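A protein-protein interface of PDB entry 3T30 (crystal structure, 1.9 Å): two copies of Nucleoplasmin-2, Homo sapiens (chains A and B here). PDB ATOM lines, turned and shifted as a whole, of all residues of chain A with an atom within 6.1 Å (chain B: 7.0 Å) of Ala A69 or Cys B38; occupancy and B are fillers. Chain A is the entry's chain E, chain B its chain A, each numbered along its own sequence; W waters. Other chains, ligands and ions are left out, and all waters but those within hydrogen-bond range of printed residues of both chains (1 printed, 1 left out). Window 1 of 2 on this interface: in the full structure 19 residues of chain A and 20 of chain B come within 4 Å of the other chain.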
ATOM      1  N   ILE A  37      30.929 -28.684  -1.136  1.00  0.00           N
ATOM      2  CA  ILE A  37      31.216 -27.570  -2.014  1.00  0.00           C
ATOM      3  C   ILE A  37      31.611 -26.423  -1.114  1.00  0.00           C
ATOM      4  O   ILE A  37      30.853 -26.084  -0.188  1.00  0.00           O
ATOM      5  CB  ILE A  37      29.949 -27.165  -2.874  1.00  0.00           C
ATOM      6  CG1 ILE A  37      29.454 -28.376  -3.691  1.00  0.00           C
ATOM      7  CG2 ILE A  37      30.295 -25.992  -3.778  1.00  0.00           C
ATOM      8  CD1 ILE A  37      28.151 -28.104  -4.563  1.00  0.00           C
ATOM      9  N   MET A  47      27.530 -13.376  -3.580  1.00  0.00           N
ATOM     10  CA  MET A  47      26.930 -14.705  -3.606  1.00  0.00           C
ATOM     11  C   MET A  47      27.454 -15.568  -4.758  1.00  0.00           C
ATOM     12  O   MET A  47      27.653 -15.079  -5.868  1.00  0.00           O
ATOM     13  CB  MET A  47      25.387 -14.633  -3.665  1.00  0.00           C
ATOM     14  CG  MET A  47      24.814 -16.022  -3.737  1.00  0.00           C
ATOM     15  SD  MET A  47      23.074 -16.379  -3.372  1.00  0.00           S
ATOM     16  CE  MET A  47      22.856 -17.495  -4.763  1.00  0.00           C
ATOM     17  N   HIS A  48      27.635 -16.866  -4.511  1.00  0.00           N
ATOM     18  CA  HIS A  48      28.124 -17.799  -5.527  1.00  0.00           C
ATOM     19  C   HIS A  48      27.045 -18.823  -5.764  1.00  0.00           C
ATOM     20  O   HIS A  48      26.410 -19.269  -4.811  1.00  0.00           O
ATOM     21  CB  HIS A  48      29.390 -18.527  -5.096  1.00  0.00           C
ATOM     22  CG  HIS A  48      30.623 -17.668  -5.093  1.00  0.00           C
ATOM     23  ND1 HIS A  48      30.766 -16.572  -4.270  1.00  0.00           N
ATOM     24  CD2 HIS A  48      31.774 -17.766  -5.807  1.00  0.00           C
ATOM     25  CE1 HIS A  48      31.954 -16.020  -4.479  1.00  0.00           C
ATOM     26  NE2 HIS A  48      32.593 -16.733  -5.393  1.00  0.00           N
ATOM     27  N   ARG A  49      26.838 -19.185  -7.027  1.00  0.00           N
ATOM     28  CA  ARG A  49      25.876 -20.218  -7.388  1.00  0.00           C
ATOM     29  C   ARG A  49      26.494 -21.230  -8.348  1.00  0.00           C
ATOM     30  O   ARG A  49      27.137 -20.861  -9.331  1.00  0.00           O
ATOM     31  CB  ARG A  49      24.628 -19.593  -8.014  1.00  0.00           C
ATOM     32  CG  ARG A  49      23.442 -20.538  -8.109  1.00  0.00           C
ATOM     33  CD  ARG A  49      22.125 -19.782  -8.025  1.00  0.00           C
ATOM     34  NE  ARG A  49      22.028 -18.739  -9.042  1.00  0.00           N
ATOM     35  CZ  ARG A  49      21.597 -18.942 -10.283  1.00  0.00           C
ATOM     36  NH1 ARG A  49      21.220 -20.155 -10.665  1.00  0.00           N
ATOM     37  NH2 ARG A  49      21.541 -17.934 -11.142  1.00  0.00           N
ATOM     38  N   VAL A  50      26.290 -22.509  -8.052  1.00  0.00           N
ATOM     39  CA  VAL A  50      26.859 -23.594  -8.841  1.00  0.00           C
ATOM     40  C   VAL A  50      25.704 -24.389  -9.392  1.00  0.00           C
ATOM     41  O   VAL A  50      24.750 -24.719  -8.669  1.00  0.00           O
ATOM     42  CB  VAL A  50      27.756 -24.514  -7.995  1.00  0.00           C
ATOM     43  CG1 VAL A  50      28.242 -25.728  -8.772  1.00  0.00           C
ATOM     44  CG2 VAL A  50      28.978 -23.702  -7.362  1.00  0.00           C
ATOM     45  N   GLU A  51      25.743 -24.616 -10.704  1.00  0.00           N
ATOM     46  CA  GLU A  51      24.684 -25.366 -11.341  1.00  0.00           C
ATOM     47  C   GLU A  51      25.283 -26.580 -11.989  1.00  0.00           C
ATOM     48  O   GLU A  51      26.502 -26.668 -12.154  1.00  0.00           O
ATOM     49  CB  GLU A  51      23.850 -24.481 -12.320  1.00  0.00           C
ATOM     50  CG  GLU A  51      24.673 -23.962 -13.501  1.00  0.00           C
ATOM     51  CD  GLU A  51      23.966 -22.806 -14.257  1.00  0.00           C
ATOM     52  OE1 GLU A  51      22.838 -22.450 -13.889  1.00  0.00           O
ATOM     53  OE2 GLU A  51      24.602 -22.241 -15.161  1.00  0.00           O
ATOM     54  N   THR A  67      20.404 -25.769 -10.354  1.00  0.00           N
ATOM     55  CA  THR A  67      21.249 -25.154  -9.317  1.00  0.00           C
ATOM     56  C   THR A  67      21.437 -26.145  -8.156  1.00  0.00           C
ATOM     57  O   THR A  67      20.444 -26.650  -7.598  1.00  0.00           O
ATOM     58  CB  THR A  67      20.570 -23.905  -8.789  1.00  0.00           C
ATOM     59  OG1 THR A  67      20.664 -22.900  -9.776  1.00  0.00           O
ATOM     60  CG2 THR A  67      21.212 -23.377  -7.491  1.00  0.00           C
ATOM     61  N   ILE A  68      22.695 -26.406  -7.769  1.00  0.00           N
ATOM     62  CA  ILE A  68      22.915 -27.323  -6.630  1.00  0.00           C
ATOM     63  C   ILE A  68      23.431 -26.670  -5.358  1.00  0.00           C
ATOM     64  O   ILE A  68      23.360 -27.280  -4.313  1.00  0.00           O
ATOM     65  CB  ILE A  68      23.835 -28.494  -6.981  1.00  0.00           C
ATOM     66  CG1 ILE A  68      25.236 -27.963  -7.395  1.00  0.00           C
ATOM     67  CG2 ILE A  68      23.164 -29.369  -8.070  1.00  0.00           C
ATOM     68  CD1 ILE A  68      26.259 -29.029  -7.682  1.00  0.00           C
ATOM     69  N   ALA A  69      23.983 -25.463  -5.448  1.00  0.00           N
ATOM     70  CA  ALA A  69      24.454 -24.808  -4.242  1.00  0.00           C
ATOM     71  C   ALA A  69      24.482 -23.308  -4.409  1.00  0.00           C
ATOM     72  O   ALA A  69      24.784 -22.822  -5.486  1.00  0.00           O
ATOM     73  CB  ALA A  69      25.867 -25.342  -3.858  1.00  0.00           C
ATOM     74  N   SER A  70      24.102 -22.604  -3.347  1.00  0.00           N
ATOM     75  CA  SER A  70      24.354 -21.170  -3.195  1.00  0.00           C
ATOM     76  C   SER A  70      25.191 -20.910  -1.921  1.00  0.00           C
ATOM     77  O   SER A  70      24.824 -21.353  -0.862  1.00  0.00           O
ATOM     78  CB  SER A  70      23.032 -20.402  -3.127  1.00  0.00           C
ATOM     79  OG  SER A  70      22.403 -20.530  -4.394  1.00  0.00           O
ATOM     80  N   LEU A  71      26.305 -20.179  -2.058  1.00  0.00           N
ATOM     81  CA  LEU A  71      27.186 -19.927  -0.954  1.00  0.00           C
ATOM     82  C   LEU A  71      27.605 -18.468  -0.951  1.00  0.00           C
ATOM     83  O   LEU A  71      27.548 -17.797  -1.988  1.00  0.00           O
ATOM     84  CB  LEU A  71      28.408 -20.836  -1.029  1.00  0.00           C
ATOM     85  CG  LEU A  71      28.190 -22.368  -1.086  1.00  0.00           C
ATOM     86  CD1 LEU A  71      29.497 -23.059  -1.477  1.00  0.00           C
ATOM     87  CD2 LEU A  71      27.657 -22.924   0.358  1.00  0.00           C
ATOM     88  N   VAL A  79      28.946 -26.232   2.053  1.00  0.00           N
ATOM     89  CA  VAL A  79      27.777 -27.068   2.325  1.00  0.00           C
ATOM     90  C   VAL A  79      28.214 -28.496   2.126  1.00  0.00           C
ATOM     91  O   VAL A  79      29.049 -28.762   1.305  1.00  0.00           O
ATOM     92  CB  VAL A  79      26.579 -26.712   1.399  1.00  0.00           C
ATOM     93  CG1 VAL A  79      26.880 -26.949  -0.105  1.00  0.00           C
ATOM     94  CG2 VAL A  79      25.274 -27.414   1.860  1.00  0.00           C
ATOM     95  N   MET A  81      26.651 -32.189   1.084  1.00  0.00           N
ATOM     96  CA  MET A  81      25.483 -32.910   0.577  1.00  0.00           C
ATOM     97  C   MET A  81      25.822 -34.373   0.388  1.00  0.00           C
ATOM     98  O   MET A  81      25.488 -34.971  -0.651  1.00  0.00           O
ATOM     99  CB  MET A  81      25.006 -32.327  -0.756  1.00  0.00           C
ATOM    100  CG  MET A  81      26.092 -32.146  -1.784  1.00  0.00           C
ATOM    101  SD  MET A  81      25.350 -31.109  -3.083  1.00  0.00           S
ATOM    102  CE  MET A  81      25.363 -29.525  -2.250  1.00  0.00           C
ATOM    103  N   THR B  36      18.869 -30.297  -2.643  1.00  0.00           N
ATOM    104  CA  THR B  36      19.167 -29.007  -2.060  1.00  0.00           C
ATOM    105  C   THR B  36      18.094 -28.016  -2.437  1.00  0.00           C
ATOM    106  O   THR B  36      17.397 -28.208  -3.416  1.00  0.00           O
ATOM    107  CB  THR B  36      20.577 -28.471  -2.496  1.00  0.00           C
ATOM    108  OG1 THR B  36      20.602 -28.214  -3.912  1.00  0.00           O
ATOM    109  CG2 THR B  36      21.704 -29.507  -2.156  1.00  0.00           C
ATOM    110  N   ILE B  37      17.980 -26.964  -1.654  1.00  0.00           N
ATOM    111  CA  ILE B  37      17.158 -25.812  -1.968  1.00  0.00           C
ATOM    112  C   ILE B  37      18.024 -24.580  -1.728  1.00  0.00           C
ATOM    113  O   ILE B  37      18.638 -24.447  -0.646  1.00  0.00           O
ATOM    114  CB  ILE B  37      15.880 -25.789  -1.050  1.00  0.00           C
ATOM    115  CG1 ILE B  37      15.054 -27.071  -1.327  1.00  0.00           C
ATOM    116  CG2 ILE B  37      15.038 -24.549  -1.397  1.00  0.00           C
ATOM    117  CD1 ILE B  37      13.802 -27.304  -0.403  1.00  0.00           C
ATOM    118  N   CYS B  38      18.090 -23.707  -2.737  1.00  0.00           N
ATOM    119  CA  CYS B  38      19.019 -22.571  -2.812  1.00  0.00           C
ATOM    120  C   CYS B  38      18.391 -21.275  -3.287  1.00  0.00           C
ATOM    121  O   CYS B  38      17.585 -21.259  -4.214  1.00  0.00           O
ATOM    122  CB  CYS B  38      20.177 -22.873  -3.782  1.00  0.00           C
ATOM    123  SG  CYS B  38      20.953 -24.466  -3.590  1.00  0.00           S
ATOM    124  N   LEU B  39      18.744 -20.185  -2.624  1.00  0.00           N
ATOM    125  CA  LEU B  39      18.304 -18.869  -3.061  1.00  0.00           C
ATOM    126  C   LEU B  39      19.164 -18.410  -4.226  1.00  0.00           C
ATOM    127  O   LEU B  39      20.348 -18.690  -4.237  1.00  0.00           O
ATOM    128  CB  LEU B  39      18.452 -17.863  -1.925  1.00  0.00           C
ATOM    129  CG  LEU B  39      17.513 -17.986  -0.736  1.00  0.00           C
ATOM    130  CD1 LEU B  39      17.828 -16.839   0.231  1.00  0.00           C
ATOM    131  CD2 LEU B  39      16.079 -17.948  -1.162  1.00  0.00           C
ATOM    132  N   GLY B  40      18.566 -17.715  -5.205  1.00  0.00           N
ATOM    133  CA  GLY B  40      19.344 -17.085  -6.269  1.00  0.00           C
ATOM    134  C   GLY B  40      19.979 -15.780  -5.805  1.00  0.00           C
ATOM    135  O   GLY B  40      19.472 -15.135  -4.886  1.00  0.00           O
ATOM    136  N   LEU B  71      14.730 -20.000   4.255  1.00  0.00           N
ATOM    137  CA  LEU B  71      16.038 -19.524   3.780  1.00  0.00           C
ATOM    138  C   LEU B  71      15.979 -18.004   3.767  1.00  0.00           C
ATOM    139  O   LEU B  71      14.896 -17.398   3.664  1.00  0.00           O
ATOM    140  CB  LEU B  71      16.345 -20.071   2.390  1.00  0.00           C
ATOM    141  CG  LEU B  71      16.451 -21.588   2.211  1.00  0.00           C
ATOM    142  CD1 LEU B  71      16.698 -21.975   0.706  1.00  0.00           C
ATOM    143  CD2 LEU B  71      17.542 -22.165   3.126  1.00  0.00           C
ATOM    144  N   PRO B  77      21.645 -19.117   2.799  1.00  0.00           N
ATOM    145  CA  PRO B  77      21.190 -19.065   1.401  1.00  0.00           C
ATOM    146  C   PRO B  77      20.829 -20.413   0.826  1.00  0.00           C
ATOM    147  O   PRO B  77      20.237 -20.472  -0.253  1.00  0.00           O
ATOM    148  CB  PRO B  77      22.402 -18.502   0.631  1.00  0.00           C
ATOM    149  CG  PRO B  77      23.608 -18.952   1.466  1.00  0.00           C
ATOM    150  CD  PRO B  77      23.113 -18.968   2.926  1.00  0.00           C
ATOM    151  N   MET B  78      21.123 -21.489   1.541  1.00  0.00           N
ATOM    152  CA  MET B  78      20.724 -22.796   1.047  1.00  0.00           C
ATOM    153  C   MET B  78      20.658 -23.835   2.115  1.00  0.00           C
ATOM    154  O   MET B  78      21.123 -23.617   3.233  1.00  0.00           O
ATOM    155  CB  MET B  78      21.717 -23.295  -0.044  1.00  0.00           C
ATOM    156  CG  MET B  78      23.042 -23.855   0.587  1.00  0.00           C
ATOM    157  SD  MET B  78      24.083 -24.666  -0.670  1.00  0.00           S
ATOM    158  CE  MET B  78      23.282 -26.214  -0.953  1.00  0.00           C
ATOM    159  N   VAL B  79      20.082 -24.984   1.765  1.00  0.00           N
ATOM    160  CA  VAL B  79      20.091 -26.104   2.660  1.00  0.00           C
ATOM    161  C   VAL B  79      20.193 -27.374   1.875  1.00  0.00           C
ATOM    162  O   VAL B  79      19.698 -27.451   0.736  1.00  0.00           O
ATOM    163  CB  VAL B  79      18.819 -26.150   3.554  1.00  0.00           C
ATOM    164  CG1 VAL B  79      17.508 -26.199   2.709  1.00  0.00           C
ATOM    165  CG2 VAL B  79      18.932 -27.290   4.641  1.00  0.00           C
ATOM    166  N   PRO B 100      14.302 -15.618  -7.001  1.00  0.00           N
ATOM    167  CA  PRO B 100      14.115 -17.046  -7.278  1.00  0.00           C
ATOM    168  C   PRO B 100      14.617 -17.988  -6.151  1.00  0.00           C
ATOM    169  O   PRO B 100      15.611 -17.690  -5.463  1.00  0.00           O
ATOM    170  CB  PRO B 100      14.953 -17.249  -8.552  1.00  0.00           C
ATOM    171  CG  PRO B 100      15.927 -16.154  -8.540  1.00  0.00           C
ATOM    172  CD  PRO B 100      15.182 -14.988  -8.013  1.00  0.00           C
ATOM    173  N   VAL B 101      13.942 -19.125  -6.003  1.00  0.00           N
ATOM    174  CA  VAL B 101      14.433 -20.199  -5.133  1.00  0.00           C
ATOM    175  C   VAL B 101      14.544 -21.386  -6.045  1.00  0.00           C
ATOM    176  O   VAL B 101      13.607 -21.661  -6.816  1.00  0.00           O
ATOM    177  CB  VAL B 101      13.397 -20.567  -4.004  1.00  0.00           C
ATOM    178  CG1 VAL B 101      13.936 -21.742  -3.163  1.00  0.00           C
ATOM    179  CG2 VAL B 101      13.086 -19.372  -3.197  1.00  0.00           C
ATOM    180  N   PHE B 102      15.669 -22.098  -5.961  1.00  0.00           N
ATOM    181  CA  PHE B 102      15.884 -23.251  -6.776  1.00  0.00           C
ATOM    182  C   PHE B 102      15.697 -24.509  -6.012  1.00  0.00           C
ATOM    183  O   PHE B 102      15.935 -24.528  -4.810  1.00  0.00           O
ATOM    184  CB  PHE B 102      17.322 -23.216  -7.362  1.00  0.00           C
ATOM    185  CG  PHE B 102      17.545 -22.059  -8.267  1.00  0.00           C
ATOM    186  CD1 PHE B 102      17.994 -20.858  -7.753  1.00  0.00           C
ATOM    187  CD2 PHE B 102      17.232 -22.150  -9.634  1.00  0.00           C
ATOM    188  CE1 PHE B 102      18.181 -19.751  -8.596  1.00  0.00           C
ATOM    189  CE2 PHE B 102      17.414 -21.063 -10.490  1.00  0.00           C
ATOM    190  CZ  PHE B 102      17.872 -19.863  -9.979  1.00  0.00           C
ATOM    191  N   LEU B 103      15.342 -25.582  -6.710  1.00  0.00           N
ATOM    192  CA  LEU B 103      15.298 -26.902  -6.083  1.00  0.00           C
ATOM    193  C   LEU B 103      16.062 -27.851  -6.977  1.00  0.00           C
ATOM    194  O   LEU B 103      16.019 -27.742  -8.189  1.00  0.00           O
ATOM    195  CB  LEU B 103      13.840 -27.405  -5.852  1.00  0.00           C
ATOM    196  CG  LEU B 103      13.031 -26.703  -4.747  1.00  0.00           C
ATOM    197  CD1 LEU B 103      12.207 -25.576  -5.317  1.00  0.00           C
ATOM    198  CD2 LEU B 103      12.125 -27.710  -4.091  1.00  0.00           C
ATOM    199  N   SER B 104      16.761 -28.801  -6.374  1.00  0.00           N
ATOM    200  CA  SER B 104      17.441 -29.819  -7.120  1.00  0.00           C
ATOM    201  C   SER B 104      17.127 -31.176  -6.554  1.00  0.00           C
ATOM    202  O   SER B 104      16.763 -31.312  -5.370  1.00  0.00           O
ATOM    203  CB  SER B 104      18.980 -29.623  -7.074  1.00  0.00           C
ATOM    204  OG  SER B 104      19.469 -29.857  -5.738  1.00  0.00           O
HETATM  205  O   HOH W   1      17.495 -25.780  -9.993  1.00  0.00           O
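The backbone NH (N) of Ser A70 lies within hydrogen-bond range of the side-chain sulfur (SG) of Cys B38, 3.7 Å away.
The backbone carbonyl oxygen of Ile A68 sits close to the side-chain sulfur of Cys B38 (3.8 Å).
SD of Met B78 is in hydrogen-bond range of N of Ser A70.
The backbone carbonyl oxygen (O) of Leu B39 sits at hydrogen-bond distance from the side-chain hydroxyl (OG) of Ser A70, 2.8 Å away.
The backbone carbonyl oxygen (O) of Ile A68 lies within hydrogen-bond range of the side-chain hydroxyl (OG1) of Thr B36 (2.9 Å).
O of Leu B39 sits close to SD of Met A47.
SG of Cys B38 sits close to N of Ala A69 (3.7 Å).
O of Pro B100 lies within hydrogen-bond range of N of Gly B40 (3.0 Å).
The backbone carbonyl oxygen (O) of Ile A37 is in hydrogen-bond range of the backbone NH (N) of Val A79 (2.9 Å).
The backbone NH (N) of Leu B39 is in hydrogen-bond range of the backbone carbonyl oxygen (O) of Pro B77 (2.8 Å).
The backbone NH of Ile A68 sits at hydrogen-bond distance from the backbone carbonyl oxygen of Val A50 (2.8 Å).
OG1 of Thr B36 sits at hydrogen-bond distance from SG of Cys B38.
The backbone NH (N) of Phe B102 lies within hydrogen-bond range of the backbone carbonyl oxygen (O) of Cys B38 (2.7 Å).
Among the printed residues, pairs that only touch across the chains: Met A47 with Gly B40 (3.5 Å), Arg A49 with Phe B102 (3.4 Å), Thr A67 with Cys B38 (3.9 Å), Thr A67 with Phe B102 (3.5 Å), Thr A67 with Ser B104 (3.4 Å), Ile A68 with Met B78 (3.5 Å), Ala A69 with Met B78 (3.6 Å), Ser A70 with Pro B77 (3.6 Å), Val A79 with Met B78 (3.6 Å) and Met A81 with Thr B36 (3.7 Å).
Printed residues of chain B within 4 Å of Met A47: Leu B39 (2.8 Å) and Gly B40 (3.5 Å).
Of chain B, only Cys B38 (3.6 Å) and Met B78 (3.6 Å) come within 4 Å of Ala A69.
Of the printed residues of chain B, Met A81 touches Thr B36.
Of the printed residues of chain A, Thr B36 touches Ile A68 and Met A81.
Printed residues of chain A within 4 Å of Cys B38: Thr A67, Ile A68, Ala A69 and Ser A70.
Printed residues of chain A within 4 Å of Met B78: Ile A68 (3.5 Å), Ala A69 (3.6 Å), Ser A70 (3.4 Å) and Val A79 (3.6 Å).
The nearest residue of chain B that does not touch Ala A69 is Thr B36 (4.6 Å).
The nearest residue of chain A that does not touch Cys B38 is Arg A49 (5.6 Å).
The nearest printed residue of chain B that does not touch Ser A70 is Gly B40 (4.8 Å).
Of the 13 printed residues of chain A, 8 touch a printed residue of chain B.
Printed residues of chain A that touch a printed residue of chain B: Met A47, Arg A49, Thr A67, Ile A68, Ala A69, Ser A70, Val A79 and Met A81.
Hydrophobic or aromatic side chains of chain A that line the printed part of chain B: Met A47, Ala A69, Val A79 and Met A81.
Hydrophobic or aromatic side chains of chain B within 4 Å of the printed part of chain A: Pro B77, Met B78 and Phe B102.
Positions printed for both chains: 37, 71 and 79.
Of the 17 pairs that touch across the chains among the printed residues, none has its exchanged pair printed and touching as well.
Water W1 bridges the backbone NH (N) of Thr A67 (2.9 Å) and the backbone carbonyl oxygen (O) of Leu B103 (3.0 Å).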
